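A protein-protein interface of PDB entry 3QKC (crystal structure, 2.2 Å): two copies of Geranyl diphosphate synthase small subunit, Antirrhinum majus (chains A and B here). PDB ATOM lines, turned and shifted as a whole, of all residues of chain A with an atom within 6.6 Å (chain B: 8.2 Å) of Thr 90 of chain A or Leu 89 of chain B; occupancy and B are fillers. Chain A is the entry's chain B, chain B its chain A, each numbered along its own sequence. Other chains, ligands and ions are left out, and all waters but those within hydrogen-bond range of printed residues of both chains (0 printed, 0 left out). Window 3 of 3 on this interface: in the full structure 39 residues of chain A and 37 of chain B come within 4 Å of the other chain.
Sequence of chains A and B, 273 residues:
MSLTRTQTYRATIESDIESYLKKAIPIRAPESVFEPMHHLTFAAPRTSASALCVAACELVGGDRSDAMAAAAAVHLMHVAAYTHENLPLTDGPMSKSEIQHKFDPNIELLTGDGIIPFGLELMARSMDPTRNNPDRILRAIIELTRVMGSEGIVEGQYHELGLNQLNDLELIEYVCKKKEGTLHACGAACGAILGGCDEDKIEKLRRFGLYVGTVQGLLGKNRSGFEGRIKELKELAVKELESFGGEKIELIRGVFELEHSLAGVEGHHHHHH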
ATOM      1  N   LEU A  87     -37.130 -15.644  15.238  1.00  0.00           N
ATOM      2  CA  LEU A  87     -35.728 -15.272  15.335  1.00  0.00           C
ATOM      3  C   LEU A  87     -34.773 -16.480  15.173  1.00  0.00           C
ATOM      4  O   LEU A  87     -34.823 -17.428  15.961  1.00  0.00           O
ATOM      5  CB  LEU A  87     -35.490 -14.575  16.664  1.00  0.00           C
ATOM      6  CG  LEU A  87     -34.079 -14.123  16.994  1.00  0.00           C
ATOM      7  CD1 LEU A  87     -33.633 -13.111  15.977  1.00  0.00           C
ATOM      8  CD2 LEU A  87     -34.083 -13.508  18.391  1.00  0.00           C
ATOM      9  N   PRO A  88     -33.903 -16.450  14.150  1.00  0.00           N
ATOM     10  CA  PRO A  88     -32.924 -17.543  13.980  1.00  0.00           C
ATOM     11  C   PRO A  88     -31.882 -17.554  15.100  1.00  0.00           C
ATOM     12  O   PRO A  88     -31.141 -16.586  15.273  1.00  0.00           O
ATOM     13  CB  PRO A  88     -32.244 -17.211  12.646  1.00  0.00           C
ATOM     14  CG  PRO A  88     -33.170 -16.293  11.952  1.00  0.00           C
ATOM     15  CD  PRO A  88     -33.826 -15.481  13.046  1.00  0.00           C
ATOM     16  N   LEU A  89     -31.836 -18.642  15.858  1.00  0.00           N
ATOM     17  CA  LEU A  89     -30.838 -18.803  16.916  1.00  0.00           C
ATOM     18  C   LEU A  89     -29.678 -19.687  16.432  1.00  0.00           C
ATOM     19  O   LEU A  89     -29.463 -19.833  15.224  1.00  0.00           O
ATOM     20  CB  LEU A  89     -31.492 -19.396  18.173  1.00  0.00           C
ATOM     21  CG  LEU A  89     -32.535 -18.523  18.891  1.00  0.00           C
ATOM     22  CD1 LEU A  89     -33.213 -19.324  19.981  1.00  0.00           C
ATOM     23  CD2 LEU A  89     -31.914 -17.240  19.448  1.00  0.00           C
ATOM     24  N   THR A  90     -28.928 -20.248  17.385  1.00  0.00           N
ATOM     25  CA  THR A  90     -27.906 -21.250  17.106  1.00  0.00           C
ATOM     26  C   THR A  90     -28.480 -22.339  16.213  1.00  0.00           C
ATOM     27  O   THR A  90     -27.932 -22.619  15.146  1.00  0.00           O
ATOM     28  CB  THR A  90     -27.315 -21.840  18.421  1.00  0.00           C
ATOM     29  OG1 THR A  90     -26.008 -21.296  18.635  1.00  0.00           O
ATOM     30  CG2 THR A  90     -27.221 -23.364  18.384  1.00  0.00           C
ATOM     31  N   ASP A  91     -29.601 -22.916  16.639  1.00  0.00           N
ATOM     32  CA  ASP A  91     -30.256 -23.995  15.908  1.00  0.00           C
ATOM     33  C   ASP A  91     -31.552 -23.541  15.209  1.00  0.00           C
ATOM     34  O   ASP A  91     -32.563 -24.251  15.221  1.00  0.00           O
ATOM     35  CB  ASP A  91     -30.508 -25.181  16.845  1.00  0.00           C
ATOM     36  CG  ASP A  91     -31.316 -24.798  18.080  1.00  0.00           C
ATOM     37  OD1 ASP A  91     -31.487 -23.588  18.357  1.00  0.00           O
ATOM     38  OD2 ASP A  91     -31.794 -25.722  18.770  1.00  0.00           O
ATOM     39  N   GLY A  92     -31.504 -22.354  14.601  1.00  0.00           N
ATOM     40  CA  GLY A  92     -32.658 -21.790  13.896  1.00  0.00           C
ATOM     41  C   GLY A  92     -33.695 -21.174  14.830  1.00  0.00           C
ATOM     42  O   GLY A  92     -33.443 -21.011  16.028  1.00  0.00           O
ATOM     43  N   PRO A 105     -30.390 -11.477  12.417  1.00  0.00           N
ATOM     44  CA  PRO A 105     -30.850 -11.923  13.725  1.00  0.00           C
ATOM     45  C   PRO A 105     -30.590 -10.925  14.862  1.00  0.00           C
ATOM     46  O   PRO A 105     -31.512 -10.638  15.632  1.00  0.00           O
ATOM     47  CB  PRO A 105     -30.071 -13.221  13.934  1.00  0.00           C
ATOM     48  CG  PRO A 105     -30.013 -13.802  12.551  1.00  0.00           C
ATOM     49  CD  PRO A 105     -29.791 -12.595  11.650  1.00  0.00           C
ATOM     50  N   ASN A 106     -29.369 -10.386  14.952  1.00  0.00           N
ATOM     51  CA  ASN A 106     -29.033  -9.481  16.056  1.00  0.00           C
ATOM     52  C   ASN A 106     -29.959  -8.266  16.111  1.00  0.00           C
ATOM     53  O   ASN A 106     -30.328  -7.816  17.194  1.00  0.00           O
ATOM     54  CB  ASN A 106     -27.540  -9.060  16.055  1.00  0.00           C
ATOM     55  CG  ASN A 106     -27.065  -8.516  14.704  1.00  0.00           C
ATOM     56  OD1 ASN A 106     -27.870  -8.173  13.841  1.00  0.00           O
ATOM     57  ND2 ASN A 106     -25.751  -8.433  14.526  1.00  0.00           N
ATOM     58  N   ILE A 107     -30.318  -7.761  14.932  1.00  0.00           N
ATOM     59  CA  ILE A 107     -31.206  -6.613  14.780  1.00  0.00           C
ATOM     60  C   ILE A 107     -32.651  -6.943  15.134  1.00  0.00           C
ATOM     61  O   ILE A 107     -33.342  -6.150  15.764  1.00  0.00           O
ATOM     62  CB  ILE A 107     -31.142  -6.070  13.321  1.00  0.00           C
ATOM     63  CG1 ILE A 107     -29.715  -5.638  12.947  1.00  0.00           C
ATOM     64  CG2 ILE A 107     -32.160  -4.950  13.076  1.00  0.00           C
ATOM     65  CD1 ILE A 107     -29.131  -4.584  13.857  1.00  0.00           C
ATOM     66  N   LEU A 109     -33.452  -9.178  17.253  1.00  0.00           N
ATOM     67  CA  LEU A 109     -33.453  -9.396  18.717  1.00  0.00           C
ATOM     68  C   LEU A 109     -33.675  -8.085  19.478  1.00  0.00           C
ATOM     69  O   LEU A 109     -34.542  -7.985  20.322  1.00  0.00           O
ATOM     70  CB  LEU A 109     -32.158 -10.064  19.183  1.00  0.00           C
ATOM     71  CG  LEU A 109     -31.866 -10.160  20.692  1.00  0.00           C
ATOM     72  CD1 LEU A 109     -32.845 -11.109  21.410  1.00  0.00           C
ATOM     73  CD2 LEU A 109     -30.443 -10.623  20.905  1.00  0.00           C
ATOM     74  N   HIS B  84     -29.915 -10.675  26.844  1.00  0.00           N
ATOM     75  CA  HIS B  84     -29.997 -10.618  25.402  1.00  0.00           C
ATOM     76  C   HIS B  84     -28.691 -10.312  24.693  1.00  0.00           C
ATOM     77  O   HIS B  84     -28.441 -10.864  23.621  1.00  0.00           O
ATOM     78  CB  HIS B  84     -31.122  -9.717  24.922  1.00  0.00           C
ATOM     79  CG  HIS B  84     -32.463 -10.353  25.047  1.00  0.00           C
ATOM     80  ND1 HIS B  84     -33.638  -9.666  24.861  1.00  0.00           N
ATOM     81  CD2 HIS B  84     -32.810 -11.625  25.352  1.00  0.00           C
ATOM     82  CE1 HIS B  84     -34.657 -10.491  25.033  1.00  0.00           C
ATOM     83  NE2 HIS B  84     -34.178 -11.685  25.330  1.00  0.00           N
ATOM     84  N   GLU B  85     -27.849  -9.471  25.274  1.00  0.00           N
ATOM     85  CA  GLU B  85     -26.591  -9.191  24.595  1.00  0.00           C
ATOM     86  C   GLU B  85     -25.559 -10.334  24.718  1.00  0.00           C
ATOM     87  O   GLU B  85     -24.632 -10.400  23.934  1.00  0.00           O
ATOM     88  CB  GLU B  85     -26.020  -7.797  24.947  1.00  0.00           C
ATOM     89  CG  GLU B  85     -25.845  -7.514  26.425  1.00  0.00           C
ATOM     90  CD  GLU B  85     -25.682  -6.005  26.741  1.00  0.00           C
ATOM     91  OE1 GLU B  85     -26.571  -5.186  26.417  1.00  0.00           O
ATOM     92  OE2 GLU B  85     -24.646  -5.657  27.342  1.00  0.00           O
ATOM     93  N   ASN B  86     -25.740 -11.231  25.685  1.00  0.00           N
ATOM     94  CA  ASN B  86     -24.881 -12.416  25.791  1.00  0.00           C
ATOM     95  C   ASN B  86     -25.524 -13.647  25.178  1.00  0.00           C
ATOM     96  O   ASN B  86     -24.974 -14.744  25.229  1.00  0.00           O
ATOM     97  CB  ASN B  86     -24.496 -12.684  27.243  1.00  0.00           C
ATOM     98  CG  ASN B  86     -23.486 -11.678  27.763  1.00  0.00           C
ATOM     99  OD1 ASN B  86     -22.286 -11.886  27.645  1.00  0.00           O
ATOM    100  ND2 ASN B  86     -23.966 -10.583  28.327  1.00  0.00           N
ATOM    101  N   LEU B  87     -26.693 -13.446  24.588  1.00  0.00           N
ATOM    102  CA  LEU B  87     -27.444 -14.523  23.983  1.00  0.00           C
ATOM    103  C   LEU B  87     -26.739 -15.056  22.721  1.00  0.00           C
ATOM    104  O   LEU B  87     -26.484 -14.291  21.785  1.00  0.00           O
ATOM    105  CB  LEU B  87     -28.835 -14.014  23.629  1.00  0.00           C
ATOM    106  CG  LEU B  87     -29.729 -15.008  22.905  1.00  0.00           C
ATOM    107  CD1 LEU B  87     -30.071 -16.140  23.842  1.00  0.00           C
ATOM    108  CD2 LEU B  87     -30.986 -14.301  22.456  1.00  0.00           C
ATOM    109  N   PRO B  88     -26.412 -16.366  22.696  1.00  0.00           N
ATOM    110  CA  PRO B  88     -25.827 -16.967  21.486  1.00  0.00           C
ATOM    111  C   PRO B  88     -26.809 -16.990  20.314  1.00  0.00           C
ATOM    112  O   PRO B  88     -27.842 -17.662  20.380  1.00  0.00           O
ATOM    113  CB  PRO B  88     -25.488 -18.403  21.927  1.00  0.00           C
ATOM    114  CG  PRO B  88     -25.373 -18.320  23.407  1.00  0.00           C
ATOM    115  CD  PRO B  88     -26.411 -17.313  23.822  1.00  0.00           C
ATOM    116  N   LEU B  89     -26.482 -16.248  19.257  1.00  0.00           N
ATOM    117  CA  LEU B  89     -27.271 -16.241  18.016  1.00  0.00           C
ATOM    118  C   LEU B  89     -26.647 -17.183  16.984  1.00  0.00           C
ATOM    119  O   LEU B  89     -25.786 -17.995  17.324  1.00  0.00           O
ATOM    120  CB  LEU B  89     -27.356 -14.818  17.441  1.00  0.00           C
ATOM    121  CG  LEU B  89     -28.147 -13.758  18.228  1.00  0.00           C
ATOM    122  CD1 LEU B  89     -27.945 -12.402  17.600  1.00  0.00           C
ATOM    123  CD2 LEU B  89     -29.630 -14.093  18.293  1.00  0.00           C
ATOM    124  N   THR B  90     -27.107 -17.070  15.736  1.00  0.00           N
ATOM    125  CA  THR B  90     -26.496 -17.746  14.590  1.00  0.00           C
ATOM    126  C   THR B  90     -25.002 -17.426  14.517  1.00  0.00           C
ATOM    127  O   THR B  90     -24.190 -18.325  14.324  1.00  0.00           O
ATOM    128  CB  THR B  90     -27.202 -17.344  13.261  1.00  0.00           C
ATOM    129  OG1 THR B  90     -28.131 -18.366  12.885  1.00  0.00           O
ATOM    130  CG2 THR B  90     -26.199 -17.142  12.120  1.00  0.00           C
ATOM    131  N   ASP B  91     -24.676 -16.147  14.717  1.00  0.00           N
ATOM    132  CA  ASP B  91     -23.324 -15.581  14.628  1.00  0.00           C
ATOM    133  C   ASP B  91     -22.707 -15.507  16.042  1.00  0.00           C
ATOM    134  O   ASP B  91     -21.653 -14.909  16.256  1.00  0.00           O
ATOM    135  CB  ASP B  91     -23.449 -14.184  13.974  1.00  0.00           C
ATOM    136  CG  ASP B  91     -22.114 -13.452  13.820  1.00  0.00           C
ATOM    137  OD1 ASP B  91     -21.671 -12.793  14.791  1.00  0.00           O
ATOM    138  OD2 ASP B  91     -21.535 -13.485  12.713  1.00  0.00           O
ATOM    139  N   GLY B  92     -23.368 -16.136  17.010  1.00  0.00           N
ATOM    140  CA  GLY B  92     -22.947 -16.026  18.406  1.00  0.00           C
ATOM    141  C   GLY B  92     -23.519 -14.783  19.069  1.00  0.00           C
ATOM    142  O   GLY B  92     -24.357 -14.108  18.476  1.00  0.00           O
ATOM    143  N   PRO B  93     -23.056 -14.456  20.292  1.00  0.00           N
ATOM    144  CA  PRO B  93     -23.694 -13.359  20.997  1.00  0.00           C
ATOM    145  C   PRO B  93     -23.252 -11.992  20.490  1.00  0.00           C
ATOM    146  O   PRO B  93     -22.249 -11.873  19.791  1.00  0.00           O
ATOM    147  CB  PRO B  93     -23.264 -13.576  22.453  1.00  0.00           C
ATOM    148  CG  PRO B  93     -21.976 -14.289  22.376  1.00  0.00           C
ATOM    149  CD  PRO B  93     -21.896 -14.980  21.035  1.00  0.00           C
ATOM    150  N   MET B  94     -24.026 -10.974  20.834  1.00  0.00           N
ATOM    151  CA  MET B  94     -23.663  -9.604  20.537  1.00  0.00           C
ATOM    152  C   MET B  94     -22.435  -9.210  21.367  1.00  0.00           C
ATOM    153  O   MET B  94     -21.569  -8.479  20.881  1.00  0.00           O
ATOM    154  CB  MET B  94     -24.846  -8.660  20.817  1.00  0.00           C
ATOM    155  CG  MET B  94     -26.067  -8.808  19.854  1.00  0.00           C
ATOM    156  SD  MET B  94     -27.310  -7.454  19.897  1.00  0.00           S
ATOM    157  CE  MET B  94     -27.697  -7.366  21.640  1.00  0.00           C
ATOM    158  N   SER B  95     -22.357  -9.708  22.602  1.00  0.00           N
ATOM    159  CA  SER B  95     -21.235  -9.423  23.498  1.00  0.00           C
ATOM    160  C   SER B  95     -20.051 -10.366  23.288  1.00  0.00           C
ATOM    161  O   SER B  95     -20.188 -11.587  23.408  1.00  0.00           O
ATOM    162  CB  SER B  95     -21.668  -9.456  24.966  1.00  0.00           C
ATOM    163  OG  SER B  95     -20.575  -9.141  25.808  1.00  0.00           O
ATOM    164  N   ASP B 104     -30.404 -22.982  27.731  1.00  0.00           N
ATOM    165  CA  ASP B 104     -30.267 -22.906  26.280  1.00  0.00           C
ATOM    166  C   ASP B 104     -30.583 -21.517  25.725  1.00  0.00           C
ATOM    167  O   ASP B 104     -31.262 -20.727  26.382  1.00  0.00           O
ATOM    168  CB  ASP B 104     -31.137 -23.969  25.613  1.00  0.00           C
ATOM    169  CG  ASP B 104     -30.523 -25.370  25.709  1.00  0.00           C
ATOM    170  OD1 ASP B 104     -29.517 -25.644  25.015  1.00  0.00           O
ATOM    171  OD2 ASP B 104     -31.063 -26.205  26.468  1.00  0.00           O
ATOM    172  N   PRO B 105     -30.073 -21.202  24.517  1.00  0.00           N
ATOM    173  CA  PRO B 105     -30.359 -19.884  23.954  1.00  0.00           C
ATOM    174  C   PRO B 105     -31.859 -19.562  23.869  1.00  0.00           C
ATOM    175  O   PRO B 105     -32.269 -18.428  24.190  1.00  0.00           O
ATOM    176  CB  PRO B 105     -29.729 -19.960  22.566  1.00  0.00           C
ATOM    177  CG  PRO B 105     -28.519 -20.873  22.773  1.00  0.00           C
ATOM    178  CD  PRO B 105     -28.990 -21.901  23.784  1.00  0.00           C
ATOM    179  N   ASN B 106     -32.673 -20.548  23.481  1.00  0.00           N
ATOM    180  CA  ASN B 106     -34.083 -20.287  23.271  1.00  0.00           C
ATOM    181  C   ASN B 106     -34.795 -19.852  24.565  1.00  0.00           C
ATOM    182  O   ASN B 106     -35.567 -18.900  24.556  1.00  0.00           O
ATOM    183  CB  ASN B 106     -34.789 -21.455  22.550  1.00  0.00           C
ATOM    184  CG  ASN B 106     -34.597 -22.790  23.239  1.00  0.00           C
ATOM    185  OD1 ASN B 106     -34.068 -22.870  24.346  1.00  0.00           O
ATOM    186  ND2 ASN B 106     -35.035 -23.851  22.581  1.00  0.00           N
ATOM    187  N   GLU B 108     -33.221 -18.492  27.299  1.00  0.00           N
ATOM    188  CA  GLU B 108     -32.710 -17.150  27.610  1.00  0.00           C
ATOM    189  C   GLU B 108     -33.442 -16.053  26.832  1.00  0.00           C
ATOM    190  O   GLU B 108     -33.578 -14.930  27.313  1.00  0.00           O
ATOM    191  CB  GLU B 108     -31.210 -17.051  27.309  1.00  0.00           C
ATOM    192  CG  GLU B 108     -30.311 -18.032  28.051  1.00  0.00           C
ATOM    193  CD  GLU B 108     -28.831 -17.697  27.902  1.00  0.00           C
ATOM    194  OE1 GLU B 108     -28.443 -17.039  26.893  1.00  0.00           O
ATOM    195  OE2 GLU B 108     -28.058 -18.056  28.811  1.00  0.00           O
ATOM    196  N   LEU B 109     -33.892 -16.376  25.626  1.00  0.00           N
ATOM    197  CA  LEU B 109     -34.617 -15.399  24.794  1.00  0.00           C
ATOM    198  C   LEU B 109     -36.021 -15.102  25.355  1.00  0.00           C
ATOM    199  O   LEU B 109     -36.404 -13.951  25.474  1.00  0.00           O
ATOM    200  CB  LEU B 109     -34.688 -15.870  23.335  1.00  0.00           C
ATOM    201  CG  LEU B 109     -35.665 -15.149  22.397  1.00  0.00           C
ATOM    202  CD1 LEU B 109     -35.193 -13.711  22.064  1.00  0.00           C
ATOM    203  CD2 LEU B 109     -35.850 -15.955  21.130  1.00  0.00           C
ATOM    204  N   LEU B 161     -23.208  -2.785  17.713  1.00  0.00           N
ATOM    205  CA  LEU B 161     -23.021  -3.741  16.629  1.00  0.00           C
ATOM    206  C   LEU B 161     -22.013  -3.180  15.640  1.00  0.00           C
ATOM    207  O   LEU B 161     -22.294  -2.203  14.939  1.00  0.00           O
ATOM    208  CB  LEU B 161     -24.354  -4.028  15.931  1.00  0.00           C
ATOM    209  CG  LEU B 161     -25.448  -4.713  16.754  1.00  0.00           C
ATOM    210  CD1 LEU B 161     -26.754  -4.628  16.016  1.00  0.00           C
ATOM    211  CD2 LEU B 161     -25.103  -6.155  17.069  1.00  0.00           C
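The backbone carbonyl oxygen (O) of Leu 89 of chain A sits at hydrogen-bond distance from the side-chain hydroxyl (OG1) of Thr 90 of chain B, 3.1 Å away.
A ring nitrogen (NE2) of His 84 of chain B lies within hydrogen-bond range of the backbone carbonyl oxygen of Leu 109 of chain B (3.2 Å).
Among the printed residues, merely in contact across the chains: Ile 107 of chain A with Leu 161 of chain B (3.2 Å), Leu 109 of chain A with His 84 of chain B (3.4 Å), Asn 106 of chain A with Leu 161 of chain B (3.5 Å), Asn 106 of chain A with Leu 89 of chain B (3.5 Å), Leu 89 of chain A with Asn 106 of chain B (3.5 Å), Thr 90 of chain A with Leu 89 of chain B (3.6 Å), Leu 109 of chain A with Leu 109 of chain B (3.6 Å), Leu 109 of chain A with Leu 87 of chain B (3.8 Å), Leu 87 of chain A with Leu 109 of chain B (3.8 Å) and Leu 89 of chain A with Leu 89 of chain B (3.97 Å).
Printed residues of chain B within 4 Å of Leu 87 of chain A: Leu 109. Printed residues of chain B within 4 Å of Thr 90 of chain A: Leu 89 (3.6 Å). Of the printed residues of chain B, Asn 106 of chain A touches Leu 89 and Leu 161. Leu 89 of chain B touches just these residues of chain A: Leu 89, Thr 90 and Asn 106. Printed residues of chain A within 4 Å of Thr 90 of chain B: Leu 89 (3.1 Å). Of the printed residues of chain A, Leu 109 of chain B touches Leu 87 (3.8 Å) and Leu 109 (3.6 Å). Printed residues of chain A within 4 Å of Leu 161 of chain B: Asn 106 and Ile 107.
Of the 10 printed residues of chain A, 6 touch a printed residue of chain B. Printed residues of chain B that touch a printed residue of chain A: His 84, Leu 87, Leu 89, Thr 90, Asn 106, Leu 109 and Leu 161. Among the printed residues, 11 pairs touch across the chains.
Leu 87 of chain A touches Leu 109 of chain B, and with the chains exchanged Leu 109 of chain A touches Leu 87 of chain B. Leu 89 of chain A touches Thr 90 of chain B, and with the chains exchanged Thr 90 of chain A touches Leu 89 of chain B. Leu 89 of chain A touches Asn 106 of chain B, and with the chains exchanged Asn 106 of chain A touches Leu 89 of chain B. Leu 109 of chain A touches its own counterpart, Leu 109 of chain B. Positions printed for both chains: 87, 88, 89, 90, 91, 92, 105, 106 and 109. Of the 11 pairs that touch across the chains among the printed residues, 8 have their exchanged pair printed and touching as well.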
